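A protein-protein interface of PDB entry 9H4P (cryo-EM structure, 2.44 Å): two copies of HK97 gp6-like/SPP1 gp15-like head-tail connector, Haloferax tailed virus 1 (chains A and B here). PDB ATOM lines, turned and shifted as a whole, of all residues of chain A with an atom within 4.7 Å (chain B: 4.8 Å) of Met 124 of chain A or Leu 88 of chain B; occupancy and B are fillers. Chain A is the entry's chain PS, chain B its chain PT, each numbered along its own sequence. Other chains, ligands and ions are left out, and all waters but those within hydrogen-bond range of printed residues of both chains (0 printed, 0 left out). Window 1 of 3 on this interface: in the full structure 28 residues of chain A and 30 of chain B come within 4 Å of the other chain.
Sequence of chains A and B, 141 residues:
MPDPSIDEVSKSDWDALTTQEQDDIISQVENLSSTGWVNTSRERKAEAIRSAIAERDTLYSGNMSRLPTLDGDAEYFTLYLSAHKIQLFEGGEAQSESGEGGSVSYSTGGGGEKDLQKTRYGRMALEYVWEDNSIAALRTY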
ATOM      1  N   TYR A  80      -0.362 -31.132   0.064  1.00  0.00           N
ATOM      2  CA  TYR A  80       0.752 -30.776   0.938  1.00  0.00           C
ATOM      3  C   TYR A  80       1.814 -31.875   0.991  1.00  0.00           C
ATOM      4  O   TYR A  80       3.001 -31.557   1.025  1.00  0.00           O
ATOM      5  CB  TYR A  80       0.285 -30.343   2.333  1.00  0.00           C
ATOM      6  CG  TYR A  80      -0.436 -29.019   2.354  1.00  0.00           C
ATOM      7  CD1 TYR A  80       0.103 -27.902   1.727  1.00  0.00           C
ATOM      8  CD2 TYR A  80      -1.655 -28.876   3.001  1.00  0.00           C
ATOM      9  CE1 TYR A  80      -0.560 -26.686   1.717  1.00  0.00           C
ATOM     10  CE2 TYR A  80      -2.330 -27.664   3.006  1.00  0.00           C
ATOM     11  CZ  TYR A  80      -1.778 -26.568   2.361  1.00  0.00           C
ATOM     12  OH  TYR A  80      -2.423 -25.366   2.354  1.00  0.00           O
ATOM     13  N   ARG A 120       7.989 -27.038   5.414  1.00  0.00           N
ATOM     14  CA  ARG A 120       6.770 -26.276   5.690  1.00  0.00           C
ATOM     15  C   ARG A 120       5.505 -27.014   5.240  1.00  0.00           C
ATOM     16  O   ARG A 120       4.515 -27.029   5.971  1.00  0.00           O
ATOM     17  CB  ARG A 120       6.873 -24.853   5.122  1.00  0.00           C
ATOM     18  CG  ARG A 120       7.045 -24.762   3.612  1.00  0.00           C
ATOM     19  CD  ARG A 120       7.794 -23.523   3.158  1.00  0.00           C
ATOM     20  NE  ARG A 120       7.730 -23.342   1.711  1.00  0.00           N
ATOM     21  CZ  ARG A 120       8.717 -23.562   0.843  1.00  0.00           C
ATOM     22  NH1 ARG A 120       8.507 -23.361  -0.446  1.00  0.00           N
ATOM     23  NH2 ARG A 120       9.902 -23.978   1.254  1.00  0.00           N
ATOM     24  N   TYR A 121       5.552 -27.625   4.048  1.00  0.00           N
ATOM     25  CA  TYR A 121       4.461 -28.428   3.510  1.00  0.00           C
ATOM     26  C   TYR A 121       4.262 -29.699   4.334  1.00  0.00           C
ATOM     27  O   TYR A 121       3.131 -30.142   4.516  1.00  0.00           O
ATOM     28  CB  TYR A 121       4.688 -28.731   2.027  1.00  0.00           C
ATOM     29  CG  TYR A 121       4.963 -27.490   1.218  1.00  0.00           C
ATOM     30  CD1 TYR A 121       3.986 -26.519   1.082  1.00  0.00           C
ATOM     31  CD2 TYR A 121       6.202 -27.265   0.635  1.00  0.00           C
ATOM     32  CE1 TYR A 121       4.225 -25.355   0.373  1.00  0.00           C
ATOM     33  CE2 TYR A 121       6.456 -26.108  -0.085  1.00  0.00           C
ATOM     34  CZ  TYR A 121       5.462 -25.152  -0.214  1.00  0.00           C
ATOM     35  OH  TYR A 121       5.707 -24.014  -0.923  1.00  0.00           O
ATOM     36  N   GLY A 122       5.369 -30.286   4.803  1.00  0.00           N
ATOM     37  CA  GLY A 122       5.319 -31.409   5.724  1.00  0.00           C
ATOM     38  C   GLY A 122       4.587 -31.045   7.013  1.00  0.00           C
ATOM     39  O   GLY A 122       3.700 -31.782   7.439  1.00  0.00           O
ATOM     40  N   ARG A 123       4.956 -29.898   7.602  1.00  0.00           N
ATOM     41  CA  ARG A 123       4.404 -29.425   8.865  1.00  0.00           C
ATOM     42  C   ARG A 123       2.919 -29.086   8.730  1.00  0.00           C
ATOM     43  O   ARG A 123       2.163 -29.300   9.678  1.00  0.00           O
ATOM     44  CB  ARG A 123       5.222 -28.258   9.426  1.00  0.00           C
ATOM     45  CG  ARG A 123       6.605 -28.673   9.907  1.00  0.00           C
ATOM     46  CD  ARG A 123       7.352 -27.598  10.667  1.00  0.00           C
ATOM     47  NE  ARG A 123       7.675 -26.445   9.840  1.00  0.00           N
ATOM     48  CZ  ARG A 123       8.847 -26.218   9.258  1.00  0.00           C
ATOM     49  NH1 ARG A 123       9.016 -25.124   8.537  1.00  0.00           N
ATOM     50  NH2 ARG A 123       9.847 -27.067   9.402  1.00  0.00           N
ATOM     51  N   MET A 124       2.510 -28.569   7.561  1.00  0.00           N
ATOM     52  CA  MET A 124       1.099 -28.331   7.290  1.00  0.00           C
ATOM     53  C   MET A 124       0.342 -29.658   7.179  1.00  0.00           C
ATOM     54  O   MET A 124      -0.718 -29.795   7.788  1.00  0.00           O
ATOM     55  CB  MET A 124       0.879 -27.457   6.052  1.00  0.00           C
ATOM     56  CG  MET A 124       1.059 -25.975   6.339  1.00  0.00           C
ATOM     57  SD  MET A 124       0.385 -24.878   5.080  1.00  0.00           S
ATOM     58  CE  MET A 124       1.632 -25.054   3.811  1.00  0.00           C
ATOM     59  N   ALA A 125       0.905 -30.633   6.449  1.00  0.00           N
ATOM     60  CA  ALA A 125       0.314 -31.957   6.293  1.00  0.00           C
ATOM     61  C   ALA A 125       0.192 -32.695   7.629  1.00  0.00           C
ATOM     62  O   ALA A 125      -0.763 -33.444   7.822  1.00  0.00           O
ATOM     63  CB  ALA A 125       1.097 -32.763   5.286  1.00  0.00           C
ATOM     64  N   LEU A 126       1.157 -32.471   8.539  1.00  0.00           N
ATOM     65  CA  LEU A 126       1.279 -33.156   9.821  1.00  0.00           C
ATOM     66  C   LEU A 126       0.080 -32.894  10.742  1.00  0.00           C
ATOM     67  O   LEU A 126      -0.291 -33.783  11.505  1.00  0.00           O
ATOM     68  CB  LEU A 126       2.616 -32.734  10.451  1.00  0.00           C
ATOM     69  CG  LEU A 126       3.053 -33.423  11.744  1.00  0.00           C
ATOM     70  CD1 LEU A 126       3.119 -34.937  11.596  1.00  0.00           C
ATOM     71  CD2 LEU A 126       4.395 -32.882  12.203  1.00  0.00           C
ATOM     72  N   GLU A 127      -0.534 -31.700  10.658  1.00  0.00           N
ATOM     73  CA  GLU A 127      -1.717 -31.344  11.439  1.00  0.00           C
ATOM     74  C   GLU A 127      -2.967 -32.130  11.011  1.00  0.00           C
ATOM     75  O   GLU A 127      -3.910 -32.219  11.795  1.00  0.00           O
ATOM     76  CB  GLU A 127      -1.969 -29.831  11.405  1.00  0.00           C
ATOM     77  CG  GLU A 127      -0.996 -29.006  12.234  1.00  0.00           C
ATOM     78  CD  GLU A 127      -1.270 -28.893  13.724  1.00  0.00           C
ATOM     79  OE1 GLU A 127      -2.241 -29.499  14.204  1.00  0.00           O
ATOM     80  OE2 GLU A 127      -0.498 -28.203  14.408  1.00  0.00           O
ATOM     81  N   TYR A 128      -2.979 -32.707   9.795  1.00  0.00           N
ATOM     82  CA  TYR A 128      -4.120 -33.452   9.262  1.00  0.00           C
ATOM     83  C   TYR A 128      -4.202 -34.870   9.836  1.00  0.00           C
ATOM     84  O   TYR A 128      -5.253 -35.504   9.740  1.00  0.00           O
ATOM     85  CB  TYR A 128      -4.059 -33.558   7.733  1.00  0.00           C
ATOM     86  CG  TYR A 128      -4.342 -32.301   6.945  1.00  0.00           C
ATOM     87  CD1 TYR A 128      -3.526 -31.185   7.056  1.00  0.00           C
ATOM     88  CD2 TYR A 128      -5.400 -32.239   6.049  1.00  0.00           C
ATOM     89  CE1 TYR A 128      -3.770 -30.032   6.327  1.00  0.00           C
ATOM     90  CE2 TYR A 128      -5.659 -31.094   5.312  1.00  0.00           C
ATOM     91  CZ  TYR A 128      -4.842 -29.988   5.454  1.00  0.00           C
ATOM     92  OH  TYR A 128      -5.088 -28.863   4.727  1.00  0.00           O
ATOM     93  N   HIS B  84      -1.261 -17.102   6.880  1.00  0.00           N
ATOM     94  CA  HIS B  84      -0.267 -18.099   7.269  1.00  0.00           C
ATOM     95  C   HIS B  84       0.154 -18.941   6.062  1.00  0.00           C
ATOM     96  O   HIS B  84       1.347 -19.112   5.826  1.00  0.00           O
ATOM     97  CB  HIS B  84      -0.745 -18.929   8.476  1.00  0.00           C
ATOM     98  CG  HIS B  84       0.101 -20.125   8.782  1.00  0.00           C
ATOM     99  ND1 HIS B  84       1.383 -20.033   9.294  1.00  0.00           N
ATOM    100  CD2 HIS B  84      -0.153 -21.442   8.646  1.00  0.00           C
ATOM    101  CE1 HIS B  84       1.878 -21.242   9.454  1.00  0.00           C
ATOM    102  NE2 HIS B  84       0.955 -22.122   9.064  1.00  0.00           N
ATOM    103  N   LYS B  85      -0.834 -19.427   5.293  1.00  0.00           N
ATOM    104  CA  LYS B  85      -0.613 -20.234   4.102  1.00  0.00           C
ATOM    105  C   LYS B  85       0.124 -19.450   3.016  1.00  0.00           C
ATOM    106  O   LYS B  85       1.110 -19.956   2.489  1.00  0.00           O
ATOM    107  CB  LYS B  85      -1.914 -20.888   3.634  1.00  0.00           C
ATOM    108  CG  LYS B  85      -2.188 -22.221   4.309  1.00  0.00           C
ATOM    109  CD  LYS B  85      -3.645 -22.514   4.518  1.00  0.00           C
ATOM    110  CE  LYS B  85      -3.867 -23.937   4.972  1.00  0.00           C
ATOM    111  NZ  LYS B  85      -2.996 -24.309   6.112  1.00  0.00           N
ATOM    112  N   ILE B  86      -0.325 -18.222   2.707  1.00  0.00           N
ATOM    113  CA  ILE B  86       0.317 -17.393   1.691  1.00  0.00           C
ATOM    114  C   ILE B  86       1.793 -17.175   2.033  1.00  0.00           C
ATOM    115  O   ILE B  86       2.648 -17.324   1.159  1.00  0.00           O
ATOM    116  CB  ILE B  86      -0.434 -16.070   1.427  1.00  0.00           C
ATOM    117  CG1 ILE B  86      -1.880 -16.320   0.990  1.00  0.00           C
ATOM    118  CG2 ILE B  86       0.306 -15.245   0.382  1.00  0.00           C
ATOM    119  CD1 ILE B  86      -2.828 -15.171   1.232  1.00  0.00           C
ATOM    120  N   GLN B  87       2.082 -16.849   3.302  1.00  0.00           N
ATOM    121  CA  GLN B  87       3.450 -16.619   3.756  1.00  0.00           C
ATOM    122  C   GLN B  87       4.315 -17.877   3.611  1.00  0.00           C
ATOM    123  O   GLN B  87       5.489 -17.762   3.260  1.00  0.00           O
ATOM    124  CB  GLN B  87       3.487 -16.023   5.166  1.00  0.00           C
ATOM    125  CG  GLN B  87       4.844 -15.440   5.555  1.00  0.00           C
ATOM    126  CD  GLN B  87       5.285 -14.292   4.679  1.00  0.00           C
ATOM    127  OE1 GLN B  87       4.501 -13.415   4.328  1.00  0.00           O
ATOM    128  NE2 GLN B  87       6.558 -14.283   4.320  1.00  0.00           N
ATOM    129  N   LEU B  88       3.739 -19.065   3.864  1.00  0.00           N
ATOM    130  CA  LEU B  88       4.441 -20.326   3.639  1.00  0.00           C
ATOM    131  C   LEU B  88       4.637 -20.623   2.151  1.00  0.00           C
ATOM    132  O   LEU B  88       5.640 -21.238   1.792  1.00  0.00           O
ATOM    133  CB  LEU B  88       3.730 -21.486   4.346  1.00  0.00           C
ATOM    134  CG  LEU B  88       3.821 -21.518   5.873  1.00  0.00           C
ATOM    135  CD1 LEU B  88       3.160 -22.769   6.418  1.00  0.00           C
ATOM    136  CD2 LEU B  88       5.262 -21.450   6.355  1.00  0.00           C
ATOM    137  N   PHE B  89       3.694 -20.200   1.292  1.00  0.00           N
ATOM    138  CA  PHE B  89       3.836 -20.353  -0.152  1.00  0.00           C
ATOM    139  C   PHE B  89       5.001 -19.501  -0.673  1.00  0.00           C
ATOM    140  O   PHE B  89       5.579 -19.834  -1.704  1.00  0.00           O
ATOM    141  CB  PHE B  89       2.518 -20.057  -0.883  1.00  0.00           C
ATOM    142  CG  PHE B  89       1.327 -20.975  -0.685  1.00  0.00           C
ATOM    143  CD1 PHE B  89       1.290 -21.982   0.277  1.00  0.00           C
ATOM    144  CD2 PHE B  89       0.192 -20.787  -1.463  1.00  0.00           C
ATOM    145  CE1 PHE B  89       0.163 -22.780   0.436  1.00  0.00           C
ATOM    146  CE2 PHE B  89      -0.933 -21.586  -1.309  1.00  0.00           C
ATOM    147  CZ  PHE B  89      -0.946 -22.580  -0.358  1.00  0.00           C
ATOM    148  N   GLU B  90       5.345 -18.421   0.055  1.00  0.00           N
ATOM    149  CA  GLU B  90       6.505 -17.577  -0.217  1.00  0.00           C
ATOM    150  C   GLU B  90       7.747 -18.007   0.580  1.00  0.00           C
ATOM    151  O   GLU B  90       8.739 -17.279   0.596  1.00  0.00           O
ATOM    152  CB  GLU B  90       6.177 -16.104   0.048  1.00  0.00           C
ATOM    153  CG  GLU B  90       5.146 -15.513  -0.899  1.00  0.00           C
ATOM    154  CD  GLU B  90       5.204 -14.007  -1.089  1.00  0.00           C
ATOM    155  OE1 GLU B  90       5.882 -13.328  -0.297  1.00  0.00           O
ATOM    156  OE2 GLU B  90       4.568 -13.515  -2.030  1.00  0.00           O
ATOM    157  N   GLY B  91       7.708 -19.170   1.247  1.00  0.00           N
ATOM    158  CA  GLY B  91       8.892 -19.747   1.878  1.00  0.00           C
ATOM    159  C   GLY B  91       9.022 -19.490   3.382  1.00  0.00           C
ATOM    160  O   GLY B  91      10.014 -19.907   3.977  1.00  0.00           O
ATOM    161  N   GLY B  92       8.040 -18.804   3.991  1.00  0.00           N
ATOM    162  CA  GLY B  92       7.986 -18.606   5.438  1.00  0.00           C
ATOM    163  C   GLY B  92       8.361 -17.188   5.874  1.00  0.00           C
ATOM    164  O   GLY B  92       8.374 -16.274   5.051  1.00  0.00           O
ATOM    165  N   ASP B 115       3.285 -26.152  13.119  1.00  0.00           N
ATOM    166  CA  ASP B 115       2.845 -25.415  11.941  1.00  0.00           C
ATOM    167  C   ASP B 115       2.517 -23.956  12.263  1.00  0.00           C
ATOM    168  O   ASP B 115       3.164 -23.060  11.722  1.00  0.00           O
ATOM    169  CB  ASP B 115       1.696 -26.153  11.244  1.00  0.00           C
ATOM    170  CG  ASP B 115       1.111 -25.437  10.040  1.00  0.00           C
ATOM    171  OD1 ASP B 115       1.883 -24.819   9.286  1.00  0.00           O
ATOM    172  OD2 ASP B 115      -0.116 -25.519   9.862  1.00  0.00           O
ATOM    173  N   THR B 119       4.997 -18.942  11.882  1.00  0.00           N
ATOM    174  CA  THR B 119       4.821 -17.608  11.299  1.00  0.00           C
ATOM    175  C   THR B 119       3.878 -16.751  12.154  1.00  0.00           C
ATOM    176  O   THR B 119       3.052 -17.297  12.882  1.00  0.00           O
ATOM    177  CB  THR B 119       4.405 -17.620   9.811  1.00  0.00           C
ATOM    178  OG1 THR B 119       2.986 -17.577   9.660  1.00  0.00           O
ATOM    179  CG2 THR B 119       4.970 -18.751   8.975  1.00  0.00           C
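Tyr 80 of chain A touches Lys 85 of chain B. Gly 91 of chain B touches Arg 120 of chain A. Leu 88 of chain B touches Tyr 121 of chain A. CB of Asp 115 of chain B touches O of Arg 123 of chain A, at 3.5 Å. Leu 88 of chain B touches Met 124 of chain A. Asp 115 of chain B touches Met 124 of chain A (OD1 to CG, 3.3 Å).
No position is printed for both chains. Of the 8 pairs that touch across the chains among the printed residues, none has its exchanged pair printed and touching as well.
A ring nitrogen (NE2) of His 84 of chain B is in hydrogen-bond range of the side-chain carboxylate (OD1) of Asp 115 of chain B. OH of Tyr 121 of chain A is in hydrogen-bond range of NH1 of Arg 120 of chain A.
Hydrophobic or aromatic side chains of chain B within 4 Å of the printed part of chain A: Leu 88. Among the printed residues, 8 pairs touch across the chains. Among the printed residues, no Asp or Glu carboxylate lies within 4 Å of a Lys or Arg side-chain nitrogen of the other chain.
The side-chain amino group (NZ) of Lys 85 of chain B lies within hydrogen-bond range of the side-chain sulfur (SD) of Met 124 of chain A, 3.6 Å away. The guanidinium group of Arg 120 of chain A sits at hydrogen-bond distance from the backbone carbonyl oxygen of Leu 88 of chain B.
Of the printed residues of chain B, Arg 120 of chain A touches Leu 88 (3.0 Å) and Gly 91 (3.8 Å). Of the printed residues of chain B, Arg 123 of chain A touches Asp 115. Of the printed residues of chain B, Tyr 121 of chain A touches Leu 88 (3.9 Å). The nearest printed residue of chain A that does not touch Leu 88 of chain B is Arg 123 of chain A (5.7 Å). The nearest printed residue of chain B that does not touch Tyr 121 of chain A is Phe 89 of chain B (4.2 Å).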
